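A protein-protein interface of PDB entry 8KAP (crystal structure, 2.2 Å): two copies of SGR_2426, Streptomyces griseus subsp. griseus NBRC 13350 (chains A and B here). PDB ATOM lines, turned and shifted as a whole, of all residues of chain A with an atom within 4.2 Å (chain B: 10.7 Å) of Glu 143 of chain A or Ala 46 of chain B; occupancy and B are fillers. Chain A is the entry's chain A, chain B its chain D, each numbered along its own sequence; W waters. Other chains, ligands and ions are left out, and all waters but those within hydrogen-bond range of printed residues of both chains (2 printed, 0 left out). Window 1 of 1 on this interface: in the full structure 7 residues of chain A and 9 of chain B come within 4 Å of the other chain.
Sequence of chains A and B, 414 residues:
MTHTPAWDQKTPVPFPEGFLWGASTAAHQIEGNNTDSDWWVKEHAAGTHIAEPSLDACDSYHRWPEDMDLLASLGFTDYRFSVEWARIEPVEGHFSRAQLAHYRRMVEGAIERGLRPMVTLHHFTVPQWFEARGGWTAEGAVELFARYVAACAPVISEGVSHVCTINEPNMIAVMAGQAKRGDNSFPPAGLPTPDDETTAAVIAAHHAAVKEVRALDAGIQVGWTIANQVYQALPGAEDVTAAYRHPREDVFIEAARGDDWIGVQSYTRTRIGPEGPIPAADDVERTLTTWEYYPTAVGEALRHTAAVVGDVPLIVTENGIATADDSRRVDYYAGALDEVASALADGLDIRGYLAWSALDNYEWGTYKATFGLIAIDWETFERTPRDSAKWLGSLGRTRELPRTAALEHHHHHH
The guanidinium group (NH1) of Arg 147 of chain A lies within hydrogen-bond range of the backbone carbonyl oxygen (O) of Thr 48 of chain B (3.0 Å).
Water W1 bridges NE2 of His 49 of chain B (2.6 Å) and O of Glu 143 of chain A (2.7 Å). Water W2 bridges NH2 of Arg 147 of chain A (2.8 Å) and N of Gly 47 of chain B (3.0 Å).
Among the printed residues, pairs that only touch across the chains: Arg 133 of chain A with Ala 46 of chain B, Glu 143 of chain A with Ala 46 of chain B, Glu 143 of chain A with Gly 47 of chain B, Leu 144 of chain A with Gly 47 of chain B, Arg 147 of chain A with Gly 47 of chain B and Arg 147 of chain A with His 49 of chain B.
O of Lys 42 of chain B sits at hydrogen-bond distance from OG1 of Thr 48 of chain B. The side-chain hydroxyl (OG1) of Thr 48 of chain B sits close to the backbone NH (N) of Ile 50 of chain B (3.2 Å).
No residue of chain B comes within 4 Å of Val 142 of chain A. Leu 144 of chain A touches just one residue of chain B: Gly 47. No residue of chain B comes within 4 Å of Ala 146 of chain A. Ala 45 of chain B touches none of the printed residues of chain A. Of chain A, only Arg 133 and Glu 143 come within 4 Å of Ala 46 of chain B. Of the printed residues of chain A, Gly 47 of chain B touches Glu 143 (3.7 Å), Leu 144 (3.6 Å) and Arg 147 (3.7 Å). Printed residues of chain A within 4 Å of His 49 of chain B: Arg 147 (3.5 Å). The nearest residue of chain B that does not touch Glu 143 of chain A is His 49 of chain B (4.4 Å). The nearest residue of chain A that does not touch Ala 46 of chain B is Gly 140 of chain A (4.1 Å).
No position is printed for both chains.
Printed residues of chain A that touch a printed residue of chain B: Arg 133, Glu 143, Leu 144 and Arg 147. Of the 17 printed residues of chain B, 4 touch a printed residue of chain A. Hydrophobic or aromatic side chains of chain B within 4 Å of the printed part of chain A: Ala 46 and His 49. Among the printed residues, 7 pairs touch across the chains. Among the printed residues, no Asp or Glu carboxylate lies within 4 Å of a Lys or Arg side-chain nitrogen of the other chain.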
ATOM      1  N   ARG A 133      -8.567  10.712 -18.933  1.00  0.00           N
ATOM      2  CA  ARG A 133      -7.851   9.490 -18.590  1.00  0.00           C
ATOM      3  C   ARG A 133      -8.533   8.262 -19.194  1.00  0.00           C
ATOM      4  O   ARG A 133      -8.025   7.153 -19.040  1.00  0.00           O
ATOM      5  CB  ARG A 133      -7.728   9.343 -17.069  1.00  0.00           C
ATOM      6  CG  ARG A 133      -9.025   8.983 -16.353  1.00  0.00           C
ATOM      7  CD  ARG A 133      -8.886   9.041 -14.842  1.00  0.00           C
ATOM      8  NE  ARG A 133      -7.851   8.142 -14.343  1.00  0.00           N
ATOM      9  CZ  ARG A 133      -7.957   6.818 -14.248  1.00  0.00           C
ATOM     10  NH1 ARG A 133      -9.111   6.211 -14.474  1.00  0.00           N
ATOM     11  NH2 ARG A 133      -6.903   6.101 -13.894  1.00  0.00           N
ATOM     12  N   GLY A 140      -9.422   1.925 -12.844  1.00  0.00           N
ATOM     13  CA  GLY A 140      -9.498   2.783 -11.672  1.00  0.00           C
ATOM     14  C   GLY A 140     -10.736   3.681 -11.659  1.00  0.00           C
ATOM     15  O   GLY A 140     -10.911   4.466 -10.729  1.00  0.00           O
ATOM     16  N   ALA A 141     -11.592   3.557 -12.682  1.00  0.00           N
ATOM     17  CA  ALA A 141     -12.759   4.417 -12.824  1.00  0.00           C
ATOM     18  C   ALA A 141     -13.748   4.162 -11.688  1.00  0.00           C
ATOM     19  O   ALA A 141     -14.302   5.104 -11.123  1.00  0.00           O
ATOM     20  CB  ALA A 141     -13.401   4.188 -14.170  1.00  0.00           C
ATOM     21  N   VAL A 142     -13.963   2.880 -11.373  1.00  0.00           N
ATOM     22  CA  VAL A 142     -14.872   2.466 -10.314  1.00  0.00           C
ATOM     23  C   VAL A 142     -14.361   2.964  -8.961  1.00  0.00           C
ATOM     24  O   VAL A 142     -15.156   3.380  -8.122  1.00  0.00           O
ATOM     25  CB  VAL A 142     -15.069   0.935 -10.331  1.00  0.00           C
ATOM     26  CG1 VAL A 142     -15.590   0.391  -9.007  1.00  0.00           C
ATOM     27  CG2 VAL A 142     -15.973   0.507 -11.477  1.00  0.00           C
ATOM     28  N   GLU A 143     -13.038   2.919  -8.753  1.00  0.00           N
ATOM     29  CA  GLU A 143     -12.451   3.325  -7.485  1.00  0.00           C
ATOM     30  C   GLU A 143     -12.563   4.841  -7.324  1.00  0.00           C
ATOM     31  O   GLU A 143     -12.826   5.324  -6.225  1.00  0.00           O
ATOM     32  CB  GLU A 143     -10.992   2.865  -7.372  1.00  0.00           C
ATOM     33  CG  GLU A 143     -10.820   1.359  -7.229  1.00  0.00           C
ATOM     34  CD  GLU A 143     -10.949   0.539  -8.503  1.00  0.00           C
ATOM     35  OE1 GLU A 143     -11.245   1.122  -9.564  1.00  0.00           O
ATOM     36  OE2 GLU A 143     -10.748  -0.689  -8.432  1.00  0.00           O
ATOM     37  N   LEU A 144     -12.362   5.582  -8.424  1.00  0.00           N
ATOM     38  CA  LEU A 144     -12.493   7.032  -8.423  1.00  0.00           C
ATOM     39  C   LEU A 144     -13.912   7.436  -8.028  1.00  0.00           C
ATOM     40  O   LEU A 144     -14.091   8.355  -7.233  1.00  0.00           O
ATOM     41  CB  LEU A 144     -12.143   7.579  -9.812  1.00  0.00           C
ATOM     42  CG  LEU A 144     -10.654   7.656 -10.146  1.00  0.00           C
ATOM     43  CD1 LEU A 144     -10.443   7.785 -11.647  1.00  0.00           C
ATOM     44  CD2 LEU A 144      -9.990   8.819  -9.424  1.00  0.00           C
ATOM     45  N   PHE A 145     -14.913   6.749  -8.596  1.00  0.00           N
ATOM     46  CA  PHE A 145     -16.304   7.092  -8.351  1.00  0.00           C
ATOM     47  C   PHE A 145     -16.673   6.818  -6.896  1.00  0.00           C
ATOM     48  O   PHE A 145     -17.343   7.633  -6.266  1.00  0.00           O
ATOM     49  CB  PHE A 145     -17.258   6.329  -9.274  1.00  0.00           C
ATOM     50  CG  PHE A 145     -18.687   6.795  -9.156  1.00  0.00           C
ATOM     51  CD1 PHE A 145     -19.033   8.087  -9.519  1.00  0.00           C
ATOM     52  CD2 PHE A 145     -19.673   5.973  -8.630  1.00  0.00           C
ATOM     53  CE1 PHE A 145     -20.338   8.536  -9.394  1.00  0.00           C
ATOM     54  CE2 PHE A 145     -20.980   6.424  -8.504  1.00  0.00           C
ATOM     55  CZ  PHE A 145     -21.310   7.704  -8.886  1.00  0.00           C
ATOM     56  N   ALA A 146     -16.239   5.663  -6.377  1.00  0.00           N
ATOM     57  CA  ALA A 146     -16.554   5.268  -5.013  1.00  0.00           C
ATOM     58  C   ALA A 146     -15.952   6.260  -4.020  1.00  0.00           C
ATOM     59  O   ALA A 146     -16.583   6.584  -3.016  1.00  0.00           O
ATOM     60  CB  ALA A 146     -16.069   3.862  -4.755  1.00  0.00           C
ATOM     61  N   ARG A 147     -14.734   6.737  -4.310  1.00  0.00           N
ATOM     62  CA  ARG A 147     -14.060   7.712  -3.466  1.00  0.00           C
ATOM     63  C   ARG A 147     -14.822   9.036  -3.477  1.00  0.00           C
ATOM     64  O   ARG A 147     -14.922   9.696  -2.444  1.00  0.00           O
ATOM     65  CB  ARG A 147     -12.613   7.935  -3.921  1.00  0.00           C
ATOM     66  CG  ARG A 147     -11.876   9.000  -3.119  1.00  0.00           C
ATOM     67  CD  ARG A 147     -10.407   9.136  -3.475  1.00  0.00           C
ATOM     68  NE  ARG A 147     -10.173   9.806  -4.748  1.00  0.00           N
ATOM     69  CZ  ARG A 147      -8.972  10.044  -5.271  1.00  0.00           C
ATOM     70  NH1 ARG A 147      -7.877   9.667  -4.635  1.00  0.00           N
ATOM     71  NH2 ARG A 147      -8.869  10.660  -6.438  1.00  0.00           N
ATOM     72  N   ASP B  38       3.347  -2.931  -1.432  1.00  0.00           N
ATOM     73  CA  ASP B  38       1.954  -2.835  -1.835  1.00  0.00           C
ATOM     74  C   ASP B  38       1.403  -1.455  -1.482  1.00  0.00           C
ATOM     75  O   ASP B  38       0.610  -0.898  -2.237  1.00  0.00           O
ATOM     76  CB  ASP B  38       1.120  -3.947  -1.192  1.00  0.00           C
ATOM     77  CG  ASP B  38       1.092  -3.903   0.326  1.00  0.00           C
ATOM     78  OD1 ASP B  38       2.160  -3.670   0.928  1.00  0.00           O
ATOM     79  OD2 ASP B  38       0.006  -4.123   0.897  1.00  0.00           O
ATOM     80  N   TRP B  39       1.836  -0.910  -0.337  1.00  0.00           N
ATOM     81  CA  TRP B  39       1.288   0.340   0.166  1.00  0.00           C
ATOM     82  C   TRP B  39       1.716   1.521  -0.700  1.00  0.00           C
ATOM     83  O   TRP B  39       0.932   2.446  -0.894  1.00  0.00           O
ATOM     84  CB  TRP B  39       1.643   0.557   1.643  1.00  0.00           C
ATOM     85  CG  TRP B  39       0.530   0.125   2.559  1.00  0.00           C
ATOM     86  CD1 TRP B  39       0.184  -1.152   2.883  1.00  0.00           C
ATOM     87  CD2 TRP B  39      -0.431   0.983   3.213  1.00  0.00           C
ATOM     88  NE1 TRP B  39      -0.901  -1.152   3.719  1.00  0.00           N
ATOM     89  CE2 TRP B  39      -1.305   0.140   3.933  1.00  0.00           C
ATOM     90  CE3 TRP B  39      -0.632   2.367   3.269  1.00  0.00           C
ATOM     91  CZ2 TRP B  39      -2.359   0.639   4.697  1.00  0.00           C
ATOM     92  CZ3 TRP B  39      -1.677   2.859   4.022  1.00  0.00           C
ATOM     93  CH2 TRP B  39      -2.530   2.005   4.721  1.00  0.00           C
ATOM     94  N   TRP B  40       2.944   1.483  -1.231  1.00  0.00           N
ATOM     95  CA  TRP B  40       3.392   2.535  -2.127  1.00  0.00           C
ATOM     96  C   TRP B  40       2.474   2.606  -3.347  1.00  0.00           C
ATOM     97  O   TRP B  40       2.039   3.693  -3.718  1.00  0.00           O
ATOM     98  CB  TRP B  40       4.860   2.349  -2.536  1.00  0.00           C
ATOM     99  CG  TRP B  40       5.402   3.518  -3.316  1.00  0.00           C
ATOM    100  CD1 TRP B  40       5.240   3.764  -4.649  1.00  0.00           C
ATOM    101  CD2 TRP B  40       6.164   4.629  -2.794  1.00  0.00           C
ATOM    102  NE1 TRP B  40       5.865   4.933  -4.996  1.00  0.00           N
ATOM    103  CE2 TRP B  40       6.436   5.488  -3.881  1.00  0.00           C
ATOM    104  CE3 TRP B  40       6.647   4.973  -1.525  1.00  0.00           C
ATOM    105  CZ2 TRP B  40       7.167   6.665  -3.733  1.00  0.00           C
ATOM    106  CZ3 TRP B  40       7.366   6.139  -1.380  1.00  0.00           C
ATOM    107  CH2 TRP B  40       7.620   6.973  -2.470  1.00  0.00           C
ATOM    108  N   VAL B  41       2.159   1.452  -3.952  1.00  0.00           N
ATOM    109  CA  VAL B  41       1.256   1.425  -5.095  1.00  0.00           C
ATOM    110  C   VAL B  41      -0.133   1.891  -4.653  1.00  0.00           C
ATOM    111  O   VAL B  41      -0.746   2.708  -5.335  1.00  0.00           O
ATOM    112  CB  VAL B  41       1.206   0.039  -5.772  1.00  0.00           C
ATOM    113  CG1 VAL B  41       0.050  -0.077  -6.757  1.00  0.00           C
ATOM    114  CG2 VAL B  41       2.519  -0.292  -6.463  1.00  0.00           C
ATOM    115  N   LYS B  42      -0.613   1.373  -3.512  1.00  0.00           N
ATOM    116  CA  LYS B  42      -1.927   1.722  -2.987  1.00  0.00           C
ATOM    117  C   LYS B  42      -2.040   3.230  -2.759  1.00  0.00           C
ATOM    118  O   LYS B  42      -3.087   3.815  -3.019  1.00  0.00           O
ATOM    119  CB  LYS B  42      -2.204   1.011  -1.657  1.00  0.00           C
ATOM    120  CG  LYS B  42      -2.610  -0.455  -1.738  1.00  0.00           C
ATOM    121  CD  LYS B  42      -2.673  -1.103  -0.365  1.00  0.00           C
ATOM    122  CE  LYS B  42      -3.540  -2.343  -0.297  1.00  0.00           C
ATOM    123  NZ  LYS B  42      -2.841  -3.544  -0.813  1.00  0.00           N
ATOM    124  N   GLU B  43      -0.957   3.841  -2.262  1.00  0.00           N
ATOM    125  CA  GLU B  43      -0.946   5.244  -1.873  1.00  0.00           C
ATOM    126  C   GLU B  43      -1.135   6.171  -3.075  1.00  0.00           C
ATOM    127  O   GLU B  43      -1.540   7.318  -2.896  1.00  0.00           O
ATOM    128  CB  GLU B  43       0.370   5.584  -1.169  1.00  0.00           C
ATOM    129  CG  GLU B  43       0.410   5.154   0.286  1.00  0.00           C
ATOM    130  CD  GLU B  43       1.809   4.992   0.853  1.00  0.00           C
ATOM    131  OE1 GLU B  43       2.669   5.843   0.554  1.00  0.00           O
ATOM    132  OE2 GLU B  43       2.033   4.026   1.604  1.00  0.00           O
ATOM    133  N   HIS B  44      -0.821   5.686  -4.284  1.00  0.00           N
ATOM    134  CA  HIS B  44      -0.834   6.519  -5.479  1.00  0.00           C
ATOM    135  C   HIS B  44      -1.745   5.941  -6.561  1.00  0.00           C
ATOM    136  O   HIS B  44      -1.747   6.440  -7.685  1.00  0.00           O
ATOM    137  CB  HIS B  44       0.587   6.674  -6.030  1.00  0.00           C
ATOM    138  CG  HIS B  44       1.535   7.309  -5.070  1.00  0.00           C
ATOM    139  ND1 HIS B  44       1.547   8.662  -4.816  1.00  0.00           N
ATOM    140  CD2 HIS B  44       2.509   6.781  -4.317  1.00  0.00           C
ATOM    141  CE1 HIS B  44       2.495   8.930  -3.928  1.00  0.00           C
ATOM    142  NE2 HIS B  44       3.090   7.801  -3.611  1.00  0.00           N
ATOM    143  N   ALA B  45      -2.516   4.897  -6.228  1.00  0.00           N
ATOM    144  CA  ALA B  45      -3.438   4.303  -7.181  1.00  0.00           C
ATOM    145  C   ALA B  45      -4.630   5.235  -7.379  1.00  0.00           C
ATOM    146  O   ALA B  45      -4.941   6.046  -6.508  1.00  0.00           O
ATOM    147  CB  ALA B  45      -3.876   2.940  -6.704  1.00  0.00           C
ATOM    148  N   ALA B  46      -5.282   5.110  -8.541  1.00  0.00           N
ATOM    149  CA  ALA B  46      -6.460   5.898  -8.864  1.00  0.00           C
ATOM    150  C   ALA B  46      -7.570   5.606  -7.857  1.00  0.00           C
ATOM    151  O   ALA B  46      -7.935   4.451  -7.650  1.00  0.00           O
ATOM    152  CB  ALA B  46      -6.913   5.591 -10.270  1.00  0.00           C
ATOM    153  N   GLY B  47      -8.087   6.668  -7.229  1.00  0.00           N
ATOM    154  CA  GLY B  47      -9.217   6.557  -6.323  1.00  0.00           C
ATOM    155  C   GLY B  47      -8.835   5.980  -4.963  1.00  0.00           C
ATOM    156  O   GLY B  47      -9.707   5.532  -4.225  1.00  0.00           O
ATOM    157  N   THR B  48      -7.535   5.988  -4.639  1.00  0.00           N
ATOM    158  CA  THR B  48      -7.074   5.568  -3.325  1.00  0.00           C
ATOM    159  C   THR B  48      -7.742   6.436  -2.262  1.00  0.00           C
ATOM    160  O   THR B  48      -7.801   7.656  -2.402  1.00  0.00           O
ATOM    161  CB  THR B  48      -5.544   5.630  -3.217  1.00  0.00           C
ATOM    162  OG1 THR B  48      -5.180   5.118  -1.934  1.00  0.00           O
ATOM    163  CG2 THR B  48      -4.974   7.023  -3.384  1.00  0.00           C
ATOM    164  N   HIS B  49      -8.244   5.792  -1.202  1.00  0.00           N
ATOM    165  CA  HIS B  49      -8.842   6.498  -0.081  1.00  0.00           C
ATOM    166  C   HIS B  49      -7.769   6.855   0.945  1.00  0.00           C
ATOM    167  O   HIS B  49      -8.078   7.454   1.972  1.00  0.00           O
ATOM    168  CB  HIS B  49      -9.952   5.659   0.565  1.00  0.00           C
ATOM    169  CG  HIS B  49     -11.141   5.420  -0.307  1.00  0.00           C
ATOM    170  ND1 HIS B  49     -12.433   5.561   0.151  1.00  0.00           N
ATOM    171  CD2 HIS B  49     -11.243   5.026  -1.581  1.00  0.00           C
ATOM    172  CE1 HIS B  49     -13.278   5.273  -0.828  1.00  0.00           C
ATOM    173  NE2 HIS B  49     -12.575   4.948  -1.890  1.00  0.00           N
ATOM    174  N   ILE B  50      -6.512   6.482   0.668  1.00  0.00           N
ATOM    175  CA  ILE B  50      -5.417   6.779   1.576  1.00  0.00           C
ATOM    176  C   ILE B  50      -5.149   8.281   1.502  1.00  0.00           C
ATOM    177  O   ILE B  50      -4.811   8.804   0.442  1.00  0.00           O
ATOM    178  CB  ILE B  50      -4.176   5.918   1.258  1.00  0.00           C
ATOM    179  CG1 ILE B  50      -4.524   4.425   1.250  1.00  0.00           C
ATOM    180  CG2 ILE B  50      -3.053   6.229   2.235  1.00  0.00           C
ATOM    181  CD1 ILE B  50      -3.371   3.501   0.916  1.00  0.00           C
ATOM    182  N   ALA B 179     -11.216  -6.245   1.818  1.00  0.00           N
ATOM    183  CA  ALA B 179     -10.770  -6.203   0.434  1.00  0.00           C
ATOM    184  C   ALA B 179     -11.524  -7.232  -0.406  1.00  0.00           C
ATOM    185  O   ALA B 179     -11.718  -7.029  -1.603  1.00  0.00           O
ATOM    186  CB  ALA B 179      -9.279  -6.422   0.368  1.00  0.00           C
ATOM    187  N   GLY B 182     -15.066  -5.486  -0.881  1.00  0.00           N
ATOM    188  CA  GLY B 182     -15.108  -4.143  -1.436  1.00  0.00           C
ATOM    189  C   GLY B 182     -15.768  -3.153  -0.478  1.00  0.00           C
ATOM    190  O   GLY B 182     -16.468  -2.240  -0.915  1.00  0.00           O
ATOM    191  N   ASP B 183     -15.543  -3.351   0.828  1.00  0.00           N
ATOM    192  CA  ASP B 183     -15.937  -2.386   1.841  1.00  0.00           C
ATOM    193  C   ASP B 183     -14.729  -1.514   2.167  1.00  0.00           C
ATOM    194  O   ASP B 183     -13.701  -2.020   2.610  1.00  0.00           O
ATOM    195  CB  ASP B 183     -16.464  -3.065   3.110  1.00  0.00           C
ATOM    196  CG  ASP B 183     -17.530  -4.119   2.863  1.00  0.00           C
ATOM    197  OD1 ASP B 183     -18.497  -3.816   2.136  1.00  0.00           O
ATOM    198  OD2 ASP B 183     -17.394  -5.227   3.418  1.00  0.00           O
ATOM    199  N   ASN B 184     -14.866  -0.203   1.933  1.00  0.00           N
ATOM    200  CA  ASN B 184     -13.787   0.747   2.154  1.00  0.00           C
ATOM    201  C   ASN B 184     -13.904   1.375   3.540  1.00  0.00           C
ATOM    202  O   ASN B 184     -12.947   1.976   4.024  1.00  0.00           O
ATOM    203  CB  ASN B 184     -13.774   1.838   1.080  1.00  0.00           C
ATOM    204  CG  ASN B 184     -13.291   1.333  -0.264  1.00  0.00           C
ATOM    205  OD1 ASN B 184     -12.199   0.778  -0.364  1.00  0.00           O
ATOM    206  ND2 ASN B 184     -14.093   1.518  -1.301  1.00  0.00           N
HETATM  207  O   HOH W   1     -12.672   3.648  -4.089  1.00  0.00           O
HETATM  208  O   HOH W   2      -6.895   9.281  -7.949  1.00  0.00           O
